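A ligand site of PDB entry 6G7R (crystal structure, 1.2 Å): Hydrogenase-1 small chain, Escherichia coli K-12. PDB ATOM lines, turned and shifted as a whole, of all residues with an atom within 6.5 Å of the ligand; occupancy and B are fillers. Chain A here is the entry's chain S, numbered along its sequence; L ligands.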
ATOM      1  N   ILE A 186     -15.422 -20.046 -12.889  1.00  0.00           N
ATOM      2  CA  ILE A 186     -15.005 -21.398 -12.535  1.00  0.00           C
ATOM      3  C   ILE A 186     -13.989 -21.917 -13.553  1.00  0.00           C
ATOM      4  O   ILE A 186     -12.931 -22.465 -13.217  1.00  0.00           O
ATOM      5  CB  ILE A 186     -16.244 -22.333 -12.436  1.00  0.00           C
ATOM      6  CG1 ILE A 186     -17.193 -21.935 -11.290  1.00  0.00           C
ATOM      7  CG2 ILE A 186     -15.859 -23.792 -12.393  1.00  0.00           C
ATOM      8  CD1 ILE A 186     -16.585 -22.046  -9.931  1.00  0.00           C
ATOM      9  N   HIS A 187     -14.345 -21.758 -14.817  1.00  0.00           N
ATOM     10  CA  HIS A 187     -13.548 -22.241 -15.973  1.00  0.00           C
ATOM     11  C   HIS A 187     -12.233 -21.469 -16.147  1.00  0.00           C
ATOM     12  O   HIS A 187     -11.378 -21.978 -16.884  1.00  0.00           O
ATOM     13  CB  HIS A 187     -14.476 -22.109 -17.193  1.00  0.00           C
ATOM     14  CG  HIS A 187     -13.990 -22.529 -18.543  1.00  0.00           C
ATOM     15  ND1 HIS A 187     -13.876 -23.840 -18.969  1.00  0.00           N
ATOM     16  CD2 HIS A 187     -13.716 -21.770 -19.615  1.00  0.00           C
ATOM     17  CE1 HIS A 187     -13.539 -23.870 -20.235  1.00  0.00           C
ATOM     18  NE2 HIS A 187     -13.425 -22.601 -20.672  1.00  0.00           N
ATOM     19  N   ASP A 188     -12.077 -20.306 -15.517  1.00  0.00           N
ATOM     20  CA  ASP A 188     -10.810 -19.593 -15.557  1.00  0.00           C
ATOM     21  C   ASP A 188      -9.780 -20.159 -14.566  1.00  0.00           C
ATOM     22  O   ASP A 188      -8.630 -19.728 -14.611  1.00  0.00           O
ATOM     23  CB  ASP A 188     -11.057 -18.103 -15.217  1.00  0.00           C
ATOM     24  CG  ASP A 188     -11.886 -17.309 -16.199  1.00  0.00           C
ATOM     25  OD1 ASP A 188     -11.974 -17.697 -17.392  1.00  0.00           O
ATOM     26  OD2 ASP A 188     -12.581 -16.314 -15.714  1.00  0.00           O
ATOM     27  N   CYS A 190     -10.103 -23.737 -13.510  1.00  0.00           N
ATOM     28  CA  CYS A 190     -10.475 -25.144 -13.377  1.00  0.00           C
ATOM     29  C   CYS A 190      -9.294 -26.067 -13.754  1.00  0.00           C
ATOM     30  O   CYS A 190      -8.643 -25.902 -14.810  1.00  0.00           O
ATOM     31  CB  CYS A 190     -11.634 -25.471 -14.311  1.00  0.00           C
ATOM     32  SG  CYS A 190     -12.171 -27.211 -14.172  1.00  0.00           S
ATOM     33  N   TYR A 191      -9.013 -27.008 -12.856  1.00  0.00           N
ATOM     34  CA  TYR A 191      -7.878 -27.939 -13.030  1.00  0.00           C
ATOM     35  C   TYR A 191      -8.098 -28.877 -14.209  1.00  0.00           C
ATOM     36  O   TYR A 191      -7.163 -29.596 -14.581  1.00  0.00           O
ATOM     37  CB  TYR A 191      -7.559 -28.676 -11.729  1.00  0.00           C
ATOM     38  CG  TYR A 191      -8.424 -29.894 -11.433  1.00  0.00           C
ATOM     39  CD1 TYR A 191      -9.815 -29.863 -11.429  1.00  0.00           C
ATOM     40  CD2 TYR A 191      -7.821 -31.110 -11.165  1.00  0.00           C
ATOM     41  CE1 TYR A 191     -10.575 -31.003 -11.182  1.00  0.00           C
ATOM     42  CE2 TYR A 191      -8.560 -32.249 -10.925  1.00  0.00           C
ATOM     43  CZ  TYR A 191      -9.946 -32.197 -10.957  1.00  0.00           C
ATOM     44  OH  TYR A 191     -10.690 -33.327 -10.778  1.00  0.00           O
ATOM     45  N   ARG A 192      -9.290 -28.912 -14.856  1.00  0.00           N
ATOM     46  CA  ARG A 192      -9.484 -29.742 -16.051  1.00  0.00           C
ATOM     47  C   ARG A 192      -9.319 -28.924 -17.337  1.00  0.00           C
ATOM     48  O   ARG A 192      -9.546 -29.478 -18.428  1.00  0.00           O
ATOM     49  CB  ARG A 192     -10.815 -30.479 -16.015  1.00  0.00           C
ATOM     50  CG  ARG A 192     -10.919 -31.414 -14.811  1.00  0.00           C
ATOM     51  CD  ARG A 192     -12.153 -32.301 -14.832  1.00  0.00           C
ATOM     52  NE  ARG A 192     -12.203 -33.141 -13.646  1.00  0.00           N
ATOM     53  CZ  ARG A 192     -12.873 -34.271 -13.522  1.00  0.00           C
ATOM     54  NH1 ARG A 192     -13.592 -34.758 -14.531  1.00  0.00           N
ATOM     55  NH2 ARG A 192     -12.852 -34.883 -12.351  1.00  0.00           N
ATOM     56  N   ARG A 193      -8.863 -27.691 -17.252  1.00  0.00           N
ATOM     57  CA  ARG A 193      -8.713 -26.866 -18.453  1.00  0.00           C
ATOM     58  C   ARG A 193      -7.690 -27.462 -19.431  1.00  0.00           C
ATOM     59  O   ARG A 193      -7.904 -27.273 -20.638  1.00  0.00           O
ATOM     60  CB  ARG A 193      -8.331 -25.441 -18.117  1.00  0.00           C
ATOM     61  CG  ARG A 193      -9.498 -24.494 -17.889  1.00  0.00           C
ATOM     62  CD  ARG A 193     -10.316 -24.227 -19.138  1.00  0.00           C
ATOM     63  NE  ARG A 193      -9.633 -23.505 -20.197  1.00  0.00           N
ATOM     64  CZ  ARG A 193      -9.800 -22.217 -20.501  1.00  0.00           C
ATOM     65  NH1 ARG A 193     -10.462 -21.417 -19.684  1.00  0.00           N
ATOM     66  NH2 ARG A 193      -9.249 -21.753 -21.602  1.00  0.00           N
ATOM     67  N   ALA A 194      -6.658 -28.149 -18.983  1.00  0.00           N
ATOM     68  CA  ALA A 194      -5.757 -28.802 -19.907  1.00  0.00           C
ATOM     69  C   ALA A 194      -6.541 -29.694 -20.880  1.00  0.00           C
ATOM     70  O   ALA A 194      -6.216 -29.779 -22.071  1.00  0.00           O
ATOM     71  CB  ALA A 194      -4.756 -29.631 -19.138  1.00  0.00           C
ATOM     72  N   HIS A 195      -7.511 -30.411 -20.335  1.00  0.00           N
ATOM     73  CA  HIS A 195      -8.292 -31.346 -21.143  1.00  0.00           C
ATOM     74  C   HIS A 195      -9.228 -30.575 -22.081  1.00  0.00           C
ATOM     75  O   HIS A 195      -9.353 -30.933 -23.258  1.00  0.00           O
ATOM     76  CB  HIS A 195      -9.055 -32.311 -20.252  1.00  0.00           C
ATOM     77  CG  HIS A 195      -8.139 -33.121 -19.381  1.00  0.00           C
ATOM     78  ND1 HIS A 195      -7.155 -33.931 -19.913  1.00  0.00           N
ATOM     79  CD2 HIS A 195      -8.059 -33.257 -18.036  1.00  0.00           C
ATOM     80  CE1 HIS A 195      -6.512 -34.506 -18.895  1.00  0.00           C
ATOM     81  NE2 HIS A 195      -7.062 -34.144 -17.738  1.00  0.00           N
ATOM     82  N   PHE A 196      -9.896 -29.530 -21.599  1.00  0.00           N
ATOM     83  CA  PHE A 196     -10.718 -28.684 -22.448  1.00  0.00           C
ATOM     84  C   PHE A 196      -9.877 -28.213 -23.631  1.00  0.00           C
ATOM     85  O   PHE A 196     -10.342 -28.297 -24.792  1.00  0.00           O
ATOM     86  CB  PHE A 196     -11.230 -27.501 -21.622  1.00  0.00           C
ATOM     87  CG  PHE A 196     -12.071 -26.528 -22.403  1.00  0.00           C
ATOM     88  CD1 PHE A 196     -13.430 -26.739 -22.576  1.00  0.00           C
ATOM     89  CD2 PHE A 196     -11.511 -25.392 -22.968  1.00  0.00           C
ATOM     90  CE1 PHE A 196     -14.194 -25.839 -23.286  1.00  0.00           C
ATOM     91  CE2 PHE A 196     -12.284 -24.474 -23.664  1.00  0.00           C
ATOM     92  CZ  PHE A 196     -13.635 -24.692 -23.817  1.00  0.00           C
ATOM     93  N   PHE A 201     -12.628 -34.888 -23.603  1.00  0.00           N
ATOM     94  CA  PHE A 201     -13.897 -34.725 -22.934  1.00  0.00           C
ATOM     95  C   PHE A 201     -14.485 -36.070 -22.500  1.00  0.00           C
ATOM     96  O   PHE A 201     -14.440 -37.056 -23.222  1.00  0.00           O
ATOM     97  CB  PHE A 201     -14.892 -34.110 -23.895  1.00  0.00           C
ATOM     98  CG  PHE A 201     -14.490 -32.755 -24.400  1.00  0.00           C
ATOM     99  CD1 PHE A 201     -14.426 -31.701 -23.529  1.00  0.00           C
ATOM    100  CD2 PHE A 201     -14.185 -32.526 -25.737  1.00  0.00           C
ATOM    101  CE1 PHE A 201     -14.051 -30.438 -23.970  1.00  0.00           C
ATOM    102  CE2 PHE A 201     -13.820 -31.265 -26.169  1.00  0.00           C
ATOM    103  CZ  PHE A 201     -13.777 -30.211 -25.291  1.00  0.00           C
ATOM    104  N   TYR A 214     -11.186 -36.208 -17.347  1.00  0.00           N
ATOM    105  CA  TYR A 214     -11.291 -35.292 -18.486  1.00  0.00           C
ATOM    106  C   TYR A 214     -12.372 -34.225 -18.263  1.00  0.00           C
ATOM    107  O   TYR A 214     -13.204 -34.288 -17.332  1.00  0.00           O
ATOM    108  CB  TYR A 214     -11.505 -36.089 -19.777  1.00  0.00           C
ATOM    109  CG  TYR A 214     -10.290 -36.776 -20.341  1.00  0.00           C
ATOM    110  CD1 TYR A 214      -9.071 -36.841 -19.689  1.00  0.00           C
ATOM    111  CD2 TYR A 214     -10.365 -37.342 -21.609  1.00  0.00           C
ATOM    112  CE1 TYR A 214      -7.965 -37.500 -20.235  1.00  0.00           C
ATOM    113  CE2 TYR A 214      -9.260 -37.948 -22.191  1.00  0.00           C
ATOM    114  CZ  TYR A 214      -8.061 -38.067 -21.495  1.00  0.00           C
ATOM    115  OH  TYR A 214      -6.985 -38.675 -22.092  1.00  0.00           O
ATOM    116  N   CYS A 215     -12.352 -33.224 -19.151  1.00  0.00           N
ATOM    117  CA  CYS A 215     -13.244 -32.077 -19.041  1.00  0.00           C
ATOM    118  C   CYS A 215     -14.704 -32.528 -19.226  1.00  0.00           C
ATOM    119  O   CYS A 215     -15.014 -33.412 -20.018  1.00  0.00           O
ATOM    120  CB  CYS A 215     -12.836 -31.041 -20.065  1.00  0.00           C
ATOM    121  SG  CYS A 215     -13.976 -29.669 -20.312  1.00  0.00           S
ATOM    122  N   LEU A 216     -15.572 -31.820 -18.513  1.00  0.00           N
ATOM    123  CA  LEU A 216     -17.009 -32.099 -18.421  1.00  0.00           C
ATOM    124  C   LEU A 216     -17.859 -31.189 -19.327  1.00  0.00           C
ATOM    125  O   LEU A 216     -19.111 -31.211 -19.240  1.00  0.00           O
ATOM    126  CB  LEU A 216     -17.454 -32.005 -16.956  1.00  0.00           C
ATOM    127  CG  LEU A 216     -16.768 -33.028 -16.071  1.00  0.00           C
ATOM    128  CD1 LEU A 216     -17.042 -32.791 -14.617  1.00  0.00           C
ATOM    129  CD2 LEU A 216     -17.124 -34.437 -16.463  1.00  0.00           C
ATOM    130  N   TYR A 217     -17.233 -30.433 -20.245  1.00  0.00           N
ATOM    131  CA  TYR A 217     -17.973 -29.521 -21.128  1.00  0.00           C
ATOM    132  C   TYR A 217     -19.094 -30.245 -21.887  1.00  0.00           C
ATOM    133  O   TYR A 217     -20.209 -29.701 -21.999  1.00  0.00           O
ATOM    134  CB  TYR A 217     -16.964 -28.885 -22.093  1.00  0.00           C
ATOM    135  CG  TYR A 217     -17.606 -28.126 -23.224  1.00  0.00           C
ATOM    136  CD1 TYR A 217     -18.227 -26.892 -23.047  1.00  0.00           C
ATOM    137  CD2 TYR A 217     -17.637 -28.672 -24.502  1.00  0.00           C
ATOM    138  CE1 TYR A 217     -18.813 -26.213 -24.111  1.00  0.00           C
ATOM    139  CE2 TYR A 217     -18.257 -28.030 -25.571  1.00  0.00           C
ATOM    140  CZ  TYR A 217     -18.841 -26.801 -25.360  1.00  0.00           C
ATOM    141  OH  TYR A 217     -19.413 -26.175 -26.429  1.00  0.00           O
ATOM    142  N   LYS A 218     -18.797 -31.397 -22.474  1.00  0.00           N
ATOM    143  CA  LYS A 218     -19.813 -32.110 -23.270  1.00  0.00           C
ATOM    144  C   LYS A 218     -20.871 -32.786 -22.396  1.00  0.00           C
ATOM    145  O   LYS A 218     -21.889 -33.206 -22.923  1.00  0.00           O
ATOM    146  CB  LYS A 218     -19.169 -33.120 -24.217  1.00  0.00           C
ATOM    147  CG  LYS A 218     -18.303 -32.469 -25.278  1.00  0.00           C
ATOM    148  CD  LYS A 218     -17.871 -33.399 -26.372  1.00  0.00           C
ATOM    149  CE  LYS A 218     -17.217 -32.622 -27.491  1.00  0.00           C
ATOM    150  NZ  LYS A 218     -16.745 -33.535 -28.553  1.00  0.00           N
ATOM    151  N   CYS A 221     -21.236 -28.978 -18.424  1.00  0.00           N
ATOM    152  CA  CYS A 221     -20.617 -28.090 -17.418  1.00  0.00           C
ATOM    153  C   CYS A 221     -20.880 -26.631 -17.763  1.00  0.00           C
ATOM    154  O   CYS A 221     -20.573 -26.183 -18.864  1.00  0.00           O
ATOM    155  CB  CYS A 221     -19.123 -28.337 -17.403  1.00  0.00           C
ATOM    156  SG  CYS A 221     -18.288 -27.413 -16.088  1.00  0.00           S
ATOM    157  N   LYS A 222     -21.361 -25.897 -16.767  1.00  0.00           N
ATOM    158  CA  LYS A 222     -21.630 -24.458 -16.919  1.00  0.00           C
ATOM    159  C   LYS A 222     -20.500 -23.612 -16.343  1.00  0.00           C
ATOM    160  O   LYS A 222     -20.622 -22.393 -16.253  1.00  0.00           O
ATOM    161  CB  LYS A 222     -23.005 -24.079 -16.364  1.00  0.00           C
ATOM    162  CG  LYS A 222     -24.129 -24.869 -17.049  1.00  0.00           C
ATOM    163  CD  LYS A 222     -24.078 -24.753 -18.575  1.00  0.00           C
ATOM    164  CE  LYS A 222     -25.169 -25.361 -19.410  1.00  0.00           C
ATOM    165  NZ  LYS A 222     -25.633 -26.674 -18.952  1.00  0.00           N
ATOM    166  N   GLY A 223     -19.346 -24.221 -16.047  1.00  0.00           N
ATOM    167  CA  GLY A 223     -18.210 -23.460 -15.570  1.00  0.00           C
ATOM    168  C   GLY A 223     -17.823 -22.274 -16.465  1.00  0.00           C
ATOM    169  O   GLY A 223     -17.432 -21.234 -15.952  1.00  0.00           O
ATOM    170  N   PRO A 224     -17.939 -22.408 -17.783  1.00  0.00           N
ATOM    171  CA  PRO A 224     -17.534 -21.310 -18.671  1.00  0.00           C
ATOM    172  C   PRO A 224     -18.360 -20.027 -18.512  1.00  0.00           C
ATOM    173  O   PRO A 224     -17.889 -18.977 -18.977  1.00  0.00           O
ATOM    174  CB  PRO A 224     -17.710 -21.880 -20.089  1.00  0.00           C
ATOM    175  CG  PRO A 224     -17.436 -23.342 -19.901  1.00  0.00           C
ATOM    176  CD  PRO A 224     -18.134 -23.651 -18.579  1.00  0.00           C
ATOM    177  N   PHE A 241     -14.899 -30.163  -5.208  1.00  0.00           N
ATOM    178  CA  PHE A 241     -15.916 -29.247  -5.752  1.00  0.00           C
ATOM    179  C   PHE A 241     -16.664 -30.065  -6.804  1.00  0.00           C
ATOM    180  O   PHE A 241     -16.234 -31.151  -7.146  1.00  0.00           O
ATOM    181  CB  PHE A 241     -15.343 -27.908  -6.264  1.00  0.00           C
ATOM    182  CG  PHE A 241     -14.594 -27.899  -7.557  1.00  0.00           C
ATOM    183  CD1 PHE A 241     -13.336 -28.478  -7.682  1.00  0.00           C
ATOM    184  CD2 PHE A 241     -15.105 -27.191  -8.637  1.00  0.00           C
ATOM    185  CE1 PHE A 241     -12.625 -28.399  -8.885  1.00  0.00           C
ATOM    186  CE2 PHE A 241     -14.383 -27.091  -9.810  1.00  0.00           C
ATOM    187  CZ  PHE A 241     -13.158 -27.704  -9.949  1.00  0.00           C
ATOM    188  N   ILE A 243     -17.004 -30.320 -10.068  1.00  0.00           N
ATOM    189  CA  ILE A 243     -16.256 -30.860 -11.195  1.00  0.00           C
ATOM    190  C   ILE A 243     -15.230 -31.900 -10.731  1.00  0.00           C
ATOM    191  O   ILE A 243     -15.042 -32.927 -11.407  1.00  0.00           O
ATOM    192  CB  ILE A 243     -15.627 -29.694 -11.975  1.00  0.00           C
ATOM    193  CG1 ILE A 243     -16.696 -28.920 -12.748  1.00  0.00           C
ATOM    194  CG2 ILE A 243     -14.481 -30.152 -12.865  1.00  0.00           C
ATOM    195  CD1 ILE A 243     -16.385 -27.444 -12.877  1.00  0.00           C
ATOM    196  N   GLY A 248     -20.471 -31.832 -13.972  1.00  0.00           N
ATOM    197  CA  GLY A 248     -20.296 -30.466 -14.403  1.00  0.00           C
ATOM    198  C   GLY A 248     -20.910 -29.461 -13.453  1.00  0.00           C
ATOM    199  O   GLY A 248     -21.894 -29.724 -12.738  1.00  0.00           O
ATOM    200  N   CYS A 249     -20.342 -28.258 -13.439  1.00  0.00           N
ATOM    201  CA  CYS A 249     -21.011 -27.125 -12.772  1.00  0.00           C
ATOM    202  C   CYS A 249     -22.450 -26.970 -13.304  1.00  0.00           C
ATOM    203  O   CYS A 249     -22.648 -27.047 -14.507  1.00  0.00           O
ATOM    204  CB  CYS A 249     -20.138 -25.892 -13.020  1.00  0.00           C
ATOM    205  SG  CYS A 249     -20.753 -24.300 -12.416  1.00  0.00           S
HETATM  206 FE1  LIG L   1     -14.140 -28.297 -18.484  1.00  0.00          FE
HETATM  207 FE2  LIG L   1     -16.119 -27.304 -16.847  1.00  0.00          FE
HETATM  208 FE3  LIG L   1     -14.298 -25.646 -18.006  1.00  0.00          FE
HETATM  209 FE4  LIG L   1     -13.526 -27.283 -16.028  1.00  0.00          FE
HETATM  210  S1  LIG L   1     -15.028 -25.511 -15.855  1.00  0.00           S
HETATM  211  S2  LIG L   1     -12.372 -26.926 -17.980  1.00  0.00           S
HETATM  212  S3  LIG L   1     -14.770 -29.177 -16.458  1.00  0.00           S
HETATM  213  S4  LIG L   1     -15.907 -26.889 -19.095  1.00  0.00           S
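Residues that only touch the ligand: Arg 192, Ile 243, Tyr 217, Gly 223, Phe 196, Pro 224 and Ile 186. Within 4 Å of the ligand: Ile 186, His 187, Cys 190, Arg 192, Arg 193, Phe 196, Cys 215, Leu 216, Tyr 217, Cys 221, Gly 223, Pro 224 and Ile 243. The nearest printed residue that does not touch the ligand is Tyr 214 (5.4 Å).
The backbone carbonyl oxygen of His 187 is in hydrogen-bond range of the guanidinium group of Arg 193 (3.0 Å). SG of Cys 215 lies close to N of Tyr 217 (3.3 Å). The guanidinium group (NH2) of Arg 192 sits at hydrogen-bond distance from the side-chain hydroxyl (OH) of Tyr 191 (3.1 Å). The backbone NH (N) of Cys 249 sits close to the side-chain sulfur (SG) of Cys 221. SG of Cys 221 lies close to N of Gly 223, at 3.4 Å. The backbone NH (N) of Arg 192 lies close to the side-chain sulfur (SG) of Cys 190, 3.4 Å away. The backbone carbonyl oxygen of Tyr 214 lies within hydrogen-bond range of the guanidinium group of Arg 192 (2.9 Å). O of Gly 223 sits close to N of His 187 (3.3 Å).
An iron atom (FE4) of the ligand is bound by the side-chain sulfur (SG) of Cys 190 (2.3 Å). A ring nitrogen (ND1) of His 187 binds an iron atom (FE3) of the ligand. SG of Cys 215 binds FE1 of the ligand (2.3 Å). N of Arg 193 lies close to S2 of the ligand. SG of Cys 221 is bound to FE2 of the ligand (2.3 Å). A sulfur (S3) of the ligand sits close to the backbone NH of Leu 216 (3.4 Å).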
